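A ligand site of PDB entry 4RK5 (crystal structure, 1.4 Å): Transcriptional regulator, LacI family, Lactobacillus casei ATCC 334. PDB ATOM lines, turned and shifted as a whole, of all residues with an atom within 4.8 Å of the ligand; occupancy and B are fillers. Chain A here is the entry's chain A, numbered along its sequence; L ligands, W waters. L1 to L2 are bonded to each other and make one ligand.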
ATOM      1  N   SER A  17       2.083   6.833 -33.809  1.00  0.00           N
ATOM      2  CA  SER A  17       1.989   7.700 -34.970  1.00  0.00           C
ATOM      3  C   SER A  17       3.327   8.251 -35.505  1.00  0.00           C
ATOM      4  O   SER A  17       3.482   8.402 -36.682  1.00  0.00           O
ATOM      5  CB  SER A  17       0.901   8.754 -34.817  1.00  0.00           C
ATOM      6  OG  SER A  17       1.255   9.673 -33.837  1.00  0.00           O
ATOM      7  N   ARG A  18       4.270   8.583 -34.620  1.00  0.00           N
ATOM      8  CA  ARG A  18       5.515   9.268 -35.048  1.00  0.00           C
ATOM      9  C   ARG A  18       6.610   9.052 -34.015  1.00  0.00           C
ATOM     10  O   ARG A  18       6.445   9.458 -32.871  1.00  0.00           O
ATOM     11  CB  ARG A  18       5.240  10.746 -35.288  1.00  0.00           C
ATOM     12  CG  ARG A  18       6.452  11.539 -35.705  1.00  0.00           C
ATOM     13  CD  ARG A  18       6.102  12.970 -36.152  1.00  0.00           C
ATOM     14  NE  ARG A  18       5.394  13.697 -35.163  1.00  0.00           N
ATOM     15  CZ  ARG A  18       5.958  14.437 -34.201  1.00  0.00           C
ATOM     16  NH1 ARG A  18       7.270  14.624 -34.111  1.00  0.00           N
ATOM     17  NH2 ARG A  18       5.164  15.053 -33.334  1.00  0.00           N
ATOM     18  N   ASN A  21       8.316  12.047 -32.159  1.00  0.00           N
ATOM     19  CA  ASN A  21       7.635  12.631 -31.008  1.00  0.00           C
ATOM     20  C   ASN A  21       8.325  12.055 -29.768  1.00  0.00           C
ATOM     21  O   ASN A  21       8.237  10.837 -29.524  1.00  0.00           O
ATOM     22  CB  ASN A  21       6.167  12.244 -31.042  1.00  0.00           C
ATOM     23  CG  ASN A  21       5.402  12.756 -29.870  1.00  0.00           C
ATOM     24  OD1 ASN A  21       5.968  13.064 -28.820  1.00  0.00           O
ATOM     25  ND2 ASN A  21       4.094  12.756 -30.004  1.00  0.00           N
ATOM     26  N   PHE A  23       7.621  11.893 -26.733  1.00  0.00           N
ATOM     27  CA  PHE A  23       6.724  11.125 -25.899  1.00  0.00           C
ATOM     28  C   PHE A  23       6.698   9.655 -26.366  1.00  0.00           C
ATOM     29  O   PHE A  23       6.823   8.716 -25.558  1.00  0.00           O
ATOM     30  CB  PHE A  23       5.316  11.711 -25.902  1.00  0.00           C
ATOM     31  CG  PHE A  23       4.310  10.795 -25.259  1.00  0.00           C
ATOM     32  CD1 PHE A  23       4.232  10.711 -23.865  1.00  0.00           C
ATOM     33  CD2 PHE A  23       3.498  10.008 -26.012  1.00  0.00           C
ATOM     34  CE1 PHE A  23       3.411   9.806 -23.304  1.00  0.00           C
ATOM     35  CE2 PHE A  23       2.658   9.092 -25.410  1.00  0.00           C
ATOM     36  CZ  PHE A  23       2.623   9.003 -24.041  1.00  0.00           C
ATOM     37  N   PHE A  24       6.523   9.454 -27.671  1.00  0.00           N
ATOM     38  CA  PHE A  24       6.468   8.086 -28.170  1.00  0.00           C
ATOM     39  C   PHE A  24       7.840   7.409 -28.095  1.00  0.00           C
ATOM     40  O   PHE A  24       7.886   6.210 -27.789  1.00  0.00           O
ATOM     41  CB  PHE A  24       5.930   8.060 -29.601  1.00  0.00           C
ATOM     42  CG  PHE A  24       4.444   8.208 -29.749  1.00  0.00           C
ATOM     43  CD1 PHE A  24       3.563   7.471 -28.969  1.00  0.00           C
ATOM     44  CD2 PHE A  24       3.903   9.081 -30.680  1.00  0.00           C
ATOM     45  CE1 PHE A  24       2.206   7.555 -29.157  1.00  0.00           C
ATOM     46  CE2 PHE A  24       2.517   9.170 -30.837  1.00  0.00           C
ATOM     47  CZ  PHE A  24       1.695   8.380 -30.078  1.00  0.00           C
ATOM     48  N   ASP A  49      -0.604   8.438 -38.880  1.00  0.00           N
ATOM     49  CA  ASP A  49      -2.110   8.453 -38.887  1.00  0.00           C
ATOM     50  C   ASP A  49      -2.756   7.787 -40.103  1.00  0.00           C
ATOM     51  O   ASP A  49      -3.941   7.977 -40.353  1.00  0.00           O
ATOM     52  CB  ASP A  49      -2.639   9.875 -38.819  1.00  0.00           C
ATOM     53  CG  ASP A  49      -2.267  10.543 -37.530  1.00  0.00           C
ATOM     54  OD1 ASP A  49      -2.161   9.821 -36.513  1.00  0.00           O
ATOM     55  OD2 ASP A  49      -2.009  11.767 -37.551  1.00  0.00           O
ATOM     56  N   ALA A  72       0.040   2.380 -29.121  1.00  0.00           N
ATOM     57  CA  ALA A  72      -0.082   3.597 -28.356  1.00  0.00           C
ATOM     58  C   ALA A  72      -0.821   4.694 -29.127  1.00  0.00           C
ATOM     59  O   ALA A  72      -0.976   5.841 -28.642  1.00  0.00           O
ATOM     60  CB  ALA A  72       1.278   4.113 -27.874  1.00  0.00           C
ATOM     61  N   SER A  73      -1.292   4.353 -30.333  1.00  0.00           N
ATOM     62  CA  SER A  73      -2.192   5.141 -31.114  1.00  0.00           C
ATOM     63  C   SER A  73      -3.038   4.181 -31.913  1.00  0.00           C
ATOM     64  O   SER A  73      -2.599   3.106 -32.227  1.00  0.00           O
ATOM     65  CB  SER A  73      -1.431   6.138 -31.944  1.00  0.00           C
ATOM     66  OG  SER A  73      -0.473   5.566 -32.715  1.00  0.00           O
ATOM     67  N   GLU A  75      -5.969   4.115 -35.208  1.00  0.00           N
ATOM     68  CA  GLU A  75      -6.618   4.799 -36.327  1.00  0.00           C
ATOM     69  C   GLU A  75      -8.008   4.279 -36.620  1.00  0.00           C
ATOM     70  O   GLU A  75      -8.946   5.065 -36.822  1.00  0.00           O
ATOM     71  CB  GLU A  75      -5.743   4.673 -37.571  1.00  0.00           C
ATOM     72  CG  GLU A  75      -4.396   5.275 -37.361  1.00  0.00           C
ATOM     73  CD  GLU A  75      -4.416   6.708 -36.740  1.00  0.00           C
ATOM     74  OE1 GLU A  75      -5.312   7.506 -37.119  1.00  0.00           O
ATOM     75  OE2 GLU A  75      -3.511   6.985 -35.850  1.00  0.00           O
ATOM     76  N   ASN A  95      -3.067   4.317 -23.756  1.00  0.00           N
ATOM     77  CA  ASN A  95      -3.093   5.775 -23.840  1.00  0.00           C
ATOM     78  C   ASN A  95      -3.561   6.320 -25.191  1.00  0.00           C
ATOM     79  O   ASN A  95      -3.112   7.373 -25.613  1.00  0.00           O
ATOM     80  CB  ASN A  95      -1.719   6.344 -23.463  1.00  0.00           C
ATOM     81  CG  ASN A  95      -1.788   7.800 -23.077  1.00  0.00           C
ATOM     82  OD1 ASN A  95      -2.760   8.242 -22.453  1.00  0.00           O
ATOM     83  ND2 ASN A  95      -0.753   8.542 -23.425  1.00  0.00           N
ATOM     84  N   HIS A 110      -7.253  12.291 -19.770  1.00  0.00           N
ATOM     85  CA  HIS A 110      -6.861  13.502 -20.442  1.00  0.00           C
ATOM     86  C   HIS A 110      -7.889  14.625 -20.409  1.00  0.00           C
ATOM     87  O   HIS A 110      -7.523  15.780 -20.386  1.00  0.00           O
ATOM     88  CB  HIS A 110      -6.408  13.212 -21.855  1.00  0.00           C
ATOM     89  CG  HIS A 110      -5.157  12.406 -21.894  1.00  0.00           C
ATOM     90  ND1 HIS A 110      -3.913  12.952 -21.658  1.00  0.00           N
ATOM     91  CD2 HIS A 110      -4.957  11.089 -22.154  1.00  0.00           C
ATOM     92  CE1 HIS A 110      -3.005  11.992 -21.766  1.00  0.00           C
ATOM     93  NE2 HIS A 110      -3.612  10.852 -22.063  1.00  0.00           N
ATOM     94  N   GLY A 134      -3.275  18.611 -32.609  1.00  0.00           N
ATOM     95  CA  GLY A 134      -2.722  17.836 -33.665  1.00  0.00           C
ATOM     96  C   GLY A 134      -3.751  17.314 -34.652  1.00  0.00           C
ATOM     97  O   GLY A 134      -3.361  16.819 -35.701  1.00  0.00           O
ATOM     98  N   GLY A 135      -5.006  17.430 -34.330  1.00  0.00           N
ATOM     99  CA  GLY A 135      -6.084  17.028 -35.204  1.00  0.00           C
ATOM    100  C   GLY A 135      -6.773  18.197 -35.853  1.00  0.00           C
ATOM    101  O   GLY A 135      -6.391  19.364 -35.695  1.00  0.00           O
ATOM    102  N   HIS A 142      -7.882  12.564 -33.293  1.00  0.00           N
ATOM    103  CA  HIS A 142      -7.092  12.271 -32.111  1.00  0.00           C
ATOM    104  C   HIS A 142      -6.922  13.451 -31.197  1.00  0.00           C
ATOM    105  O   HIS A 142      -6.724  14.624 -31.610  1.00  0.00           O
ATOM    106  CB  HIS A 142      -5.734  11.727 -32.446  1.00  0.00           C
ATOM    107  CG  HIS A 142      -5.802  10.509 -33.272  1.00  0.00           C
ATOM    108  ND1 HIS A 142      -6.917  10.156 -34.000  1.00  0.00           N
ATOM    109  CD2 HIS A 142      -4.868   9.560 -33.525  1.00  0.00           C
ATOM    110  CE1 HIS A 142      -6.665   9.020 -34.632  1.00  0.00           C
ATOM    111  NE2 HIS A 142      -5.432   8.656 -34.384  1.00  0.00           N
ATOM    112  N   GLY A 143      -7.015  13.121 -29.934  1.00  0.00           N
ATOM    113  CA  GLY A 143      -6.950  14.163 -28.861  1.00  0.00           C
ATOM    114  C   GLY A 143      -8.282  14.894 -28.705  1.00  0.00           C
ATOM    115  O   GLY A 143      -8.351  15.994 -28.215  1.00  0.00           O
ATOM    116  N   ARG A 146      -9.478  16.058 -25.211  1.00  0.00           N
ATOM    117  CA  ARG A 146      -8.865  17.335 -24.872  1.00  0.00           C
ATOM    118  C   ARG A 146      -9.614  18.540 -25.495  1.00  0.00           C
ATOM    119  O   ARG A 146      -9.833  19.555 -24.857  1.00  0.00           O
ATOM    120  CB  ARG A 146      -7.398  17.372 -25.229  1.00  0.00           C
ATOM    121  CG  ARG A 146      -6.625  16.246 -24.615  1.00  0.00           C
ATOM    122  CD  ARG A 146      -5.260  16.293 -25.074  1.00  0.00           C
ATOM    123  NE  ARG A 146      -4.561  15.089 -24.785  1.00  0.00           N
ATOM    124  CZ  ARG A 146      -3.248  14.920 -25.040  1.00  0.00           C
ATOM    125  NH1 ARG A 146      -2.514  15.943 -25.506  1.00  0.00           N
ATOM    126  NH2 ARG A 146      -2.661  13.789 -24.803  1.00  0.00           N
ATOM    127  N   HIS A 171       1.852  19.719 -35.052  1.00  0.00           N
ATOM    128  CA  HIS A 171       2.520  18.602 -34.378  1.00  0.00           C
ATOM    129  C   HIS A 171       3.928  18.892 -33.913  1.00  0.00           C
ATOM    130  O   HIS A 171       4.348  18.440 -32.826  1.00  0.00           O
ATOM    131  CB  HIS A 171       2.591  17.392 -35.324  1.00  0.00           C
ATOM    132  CG  HIS A 171       1.297  16.935 -35.836  1.00  0.00           C
ATOM    133  ND1 HIS A 171       0.898  17.105 -37.128  1.00  0.00           N
ATOM    134  CD2 HIS A 171       0.255  16.382 -35.199  1.00  0.00           C
ATOM    135  CE1 HIS A 171      -0.349  16.657 -37.250  1.00  0.00           C
ATOM    136  NE2 HIS A 171      -0.746  16.215 -36.094  1.00  0.00           N
ATOM    137  N   ASN A 198      -1.064  21.481 -26.567  1.00  0.00           N
ATOM    138  CA  ASN A 198      -1.248  20.039 -26.723  1.00  0.00           C
ATOM    139  C   ASN A 198       0.043  19.258 -26.957  1.00  0.00           C
ATOM    140  O   ASN A 198      -0.023  18.040 -27.224  1.00  0.00           O
ATOM    141  CB  ASN A 198      -2.311  19.718 -27.775  1.00  0.00           C
ATOM    142  CG  ASN A 198      -3.630  19.374 -27.181  1.00  0.00           C
ATOM    143  OD1 ASN A 198      -3.716  18.550 -26.263  1.00  0.00           O
ATOM    144  ND2 ASN A 198      -4.690  19.994 -27.665  1.00  0.00           N
ATOM    145  N   SER A 199       1.205  19.896 -26.804  1.00  0.00           N
ATOM    146  CA  SER A 199       2.436  19.175 -27.100  1.00  0.00           C
ATOM    147  C   SER A 199       3.629  20.056 -26.715  1.00  0.00           C
ATOM    148  O   SER A 199       3.757  21.216 -27.110  1.00  0.00           O
ATOM    149  CB  SER A 199       2.567  18.956 -28.616  1.00  0.00           C
ATOM    150  OG  SER A 199       3.909  18.761 -29.000  1.00  0.00           O
ATOM    151  N   TYR A 226       2.318  20.044 -23.265  1.00  0.00           N
ATOM    152  CA  TYR A 226       1.679  18.795 -22.866  1.00  0.00           C
ATOM    153  C   TYR A 226       2.681  17.679 -23.030  1.00  0.00           C
ATOM    154  O   TYR A 226       3.334  17.577 -24.081  1.00  0.00           O
ATOM    155  CB  TYR A 226       0.431  18.480 -23.716  1.00  0.00           C
ATOM    156  CG  TYR A 226      -0.672  17.716 -22.994  1.00  0.00           C
ATOM    157  CD1 TYR A 226      -0.544  16.362 -22.699  1.00  0.00           C
ATOM    158  CD2 TYR A 226      -1.835  18.310 -22.612  1.00  0.00           C
ATOM    159  CE1 TYR A 226      -1.548  15.684 -22.047  1.00  0.00           C
ATOM    160  CE2 TYR A 226      -2.880  17.653 -22.028  1.00  0.00           C
ATOM    161  CZ  TYR A 226      -2.724  16.321 -21.712  1.00  0.00           C
ATOM    162  OH  TYR A 226      -3.755  15.651 -21.104  1.00  0.00           O
ATOM    163  N   ASP A 227       2.818  16.872 -21.986  1.00  0.00           N
ATOM    164  CA  ASP A 227       3.509  15.561 -21.909  1.00  0.00           C
ATOM    165  C   ASP A 227       4.592  15.542 -20.818  1.00  0.00           C
ATOM    166  O   ASP A 227       4.756  14.501 -20.170  1.00  0.00           O
ATOM    167  CB  ASP A 227       4.174  15.075 -23.188  1.00  0.00           C
ATOM    168  CG  ASP A 227       3.204  14.742 -24.320  1.00  0.00           C
ATOM    169  OD1 ASP A 227       1.993  14.635 -24.075  1.00  0.00           O
ATOM    170  OD2 ASP A 227       3.757  14.586 -25.420  1.00  0.00           O
ATOM    171  N   GLN A 229       7.934  16.096 -21.691  1.00  0.00           N
ATOM    172  CA  GLN A 229       8.953  15.420 -22.448  1.00  0.00           C
ATOM    173  C   GLN A 229      10.352  15.693 -21.875  1.00  0.00           C
ATOM    174  O   GLN A 229      10.542  16.635 -21.120  1.00  0.00           O
ATOM    175  CB  GLN A 229       8.889  15.826 -23.936  1.00  0.00           C
ATOM    176  CG  GLN A 229       7.593  15.361 -24.564  1.00  0.00           C
ATOM    177  CD  GLN A 229       7.386  15.846 -25.985  1.00  0.00           C
ATOM    178  OE1 GLN A 229       8.301  16.372 -26.629  1.00  0.00           O
ATOM    179  NE2 GLN A 229       6.170  15.656 -26.489  1.00  0.00           N
ATOM    180  N   GLN A 244       2.770  13.330 -18.286  1.00  0.00           N
ATOM    181  CA  GLN A 244       2.296  11.958 -18.512  1.00  0.00           C
ATOM    182  C   GLN A 244       3.251  10.981 -17.832  1.00  0.00           C
ATOM    183  O   GLN A 244       4.467  11.105 -17.972  1.00  0.00           O
ATOM    184  CB  GLN A 244       2.187  11.634 -20.003  1.00  0.00           C
ATOM    185  CG  GLN A 244       1.150  12.485 -20.728  1.00  0.00           C
ATOM    186  CD  GLN A 244       0.536  11.778 -21.907  1.00  0.00           C
ATOM    187  OE1 GLN A 244      -0.037  10.693 -21.721  1.00  0.00           O
ATOM    188  NE2 GLN A 244       0.618  12.366 -23.070  1.00  0.00           N
HETATM  189  C1  LIG L   1       0.335  11.653 -29.151  1.00  0.00           C
HETATM  190  C2  LIG L   1       0.054  11.002 -27.803  1.00  0.00           C
HETATM  191  C3  LIG L   1      -0.509  11.987 -26.795  1.00  0.00           C
HETATM  192  C4  LIG L   1       0.504  13.116 -26.672  1.00  0.00           C
HETATM  193  C5  LIG L   1       0.650  13.764 -28.049  1.00  0.00           C
HETATM  194  C6  LIG L   1       1.633  14.916 -28.134  1.00  0.00           C
HETATM  195  O1  LIG L   1      -0.860   9.889 -28.008  1.00  0.00           O
HETATM  196  O2  LIG L   1      -0.660  11.338 -25.528  1.00  0.00           O
HETATM  197  O3  LIG L   1       0.033  14.106 -25.749  1.00  0.00           O
HETATM  198  O4  LIG L   1       1.153  12.786 -29.008  1.00  0.00           O
HETATM  199  O5  LIG L   1       2.983  14.476 -27.864  1.00  0.00           O
HETATM  200  C1  LG2 L   2      -1.586  10.302 -31.342  1.00  0.00           C
HETATM  201  C2  LG2 L   2      -1.064  11.722 -31.143  1.00  0.00           C
HETATM  202  C3  LG2 L   2      -1.910  12.842 -31.733  1.00  0.00           C
HETATM  203  C4  LG2 L   2      -0.874  13.939 -31.912  1.00  0.00           C
HETATM  204  C5  LG2 L   2       0.287  13.138 -32.473  1.00  0.00           C
HETATM  205  C6  LG2 L   2       1.644  13.722 -32.216  1.00  0.00           C
HETATM  206  O1  LG2 L   2      -1.620   9.950 -32.738  1.00  0.00           O
HETATM  207  O2  LG2 L   2      -0.936  12.014 -29.740  1.00  0.00           O
HETATM  208  O3  LG2 L   2      -3.024  13.178 -30.888  1.00  0.00           O
HETATM  209  O4  LG2 L   2      -1.298  14.957 -32.806  1.00  0.00           O
HETATM  210  O5  LG2 L   2       0.185  11.839 -31.815  1.00  0.00           O
HETATM  211  O6  LG2 L   2       2.724  12.955 -32.704  1.00  0.00           O
HETATM  212  O   HOH W   1       0.069  17.183 -31.088  1.00  0.00           O
HETATM  213  O   HOH W   2      -3.203  10.220 -25.485  1.00  0.00           O
HETATM  214  O   HOH W   3      -2.984   7.850 -29.173  1.00  0.00           O
HETATM  215  O   HOH W   4      -3.134  14.119 -28.377  1.00  0.00           O
HETATM  216  O   HOH W   5      -2.281  12.873 -35.230  1.00  0.00           O
HETATM  217  O   HOH W   6      -0.476   7.580 -26.560  1.00  0.00           O
HETATM  218  O   HOH W   7       4.579  16.205 -29.165  1.00  0.00           O
HETATM  219  O   HOH W   8      -3.650  10.628 -28.237  1.00  0.00           O
HETATM  220  O   HOH W   9       2.805  16.733 -31.455  1.00  0.00           O
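The side-chain carboxylate (OD2) of Asp 227 sits at hydrogen-bond distance from an oxygen (O5) of LIG L1.
The guanidinium group of Arg 146 lies within hydrogen-bond range of an oxygen (O3) of LIG L1 (2.9 Å).
The side-chain amide nitrogen (NE2) of Gln 244 lies within hydrogen-bond range of an oxygen (O2) of LIG L1.
The side-chain amide nitrogen (ND2) of Asn 21 is in hydrogen-bond range of an oxygen (O5) of LIG L1 (3.0 Å).
The side-chain hydroxyl (OG) of Ser 17 is in hydrogen-bond range of an oxygen (O1) of LG2 L2.
The guanidinium group of Arg 18 sits at hydrogen-bond distance from an oxygen (O6) of LG2 L2 (3.3 Å).
An oxygen (O2) of LIG L1 sits at hydrogen-bond distance from the side-chain amide nitrogen of Asn 95 (3.5 Å).
The side-chain amide nitrogen of Gln 229 sits at hydrogen-bond distance from the side-chain carboxylate of Asp 227 (2.8 Å).
NH1 of Arg 146 sits at hydrogen-bond distance from OD1 of Asn 198.
The side-chain amide nitrogen (NE2) of Gln 229 is in hydrogen-bond range of the side-chain amide oxygen (OD1) of Asn 21 (3.5 Å).
The backbone NH (N) of Phe 23 sits at hydrogen-bond distance from the side-chain amide oxygen (OD1) of Asn 21, 2.9 Å away.
N of Ser 17 sits at hydrogen-bond distance from OG of Ser 73 (3.1 Å).
A ring nitrogen (NE2) of His 171 sits at hydrogen-bond distance from the backbone carbonyl oxygen of Gly 134.
OE2 of Glu 75 lies within hydrogen-bond range of NE2 of His 142.
OH of Tyr 226 sits at hydrogen-bond distance from ND1 of His 110 (2.8 Å).
Merely in contact with the ligand: Phe 24 (3.6 Å), Asp 49 (3.8 Å), Ser 73 (3.9 Å), Gly 134 (3.3 Å), His 142 (3.4 Å), His 171 (3.2 Å), Asn 198 (3.7 Å), Tyr 226 (3.8 Å) and Gln 229 (3.7 Å).
Hydrophobic or aromatic side chains that line the ligand: Phe 24, His 142, His 171 and Tyr 226.
Water W4 bridges an oxygen (O3) of LG2 L2 (2.7 Å) and the guanidinium group (NH1) of Arg 146 (3.5 Å).
Water W7 lies within hydrogen-bond range of the side-chain hydroxyl (OG) of Ser 199 (2.6 Å), an oxygen (O5) of LIG L1 (2.7 Å), the side-chain amide nitrogen (NE2) of Gln 229 (3.2 Å) and the side-chain amide oxygen (OD1) of Asn 21 (3.5 Å).
Water W2 lies within hydrogen-bond range of O2 of LIG L1 and O of Asn 95.
Water W3 bridges the backbone carbonyl oxygen of Ala 72 and an oxygen (O1) of LIG L1.
Water W9 lies within hydrogen-bond range of the backbone carbonyl oxygen of His 171, the side-chain hydroxyl of Ser 199 and the guanidinium group of Arg 18.
Water W5 bridges the side-chain carboxylate of Asp 49 and an oxygen (O4) of LG2 L2.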
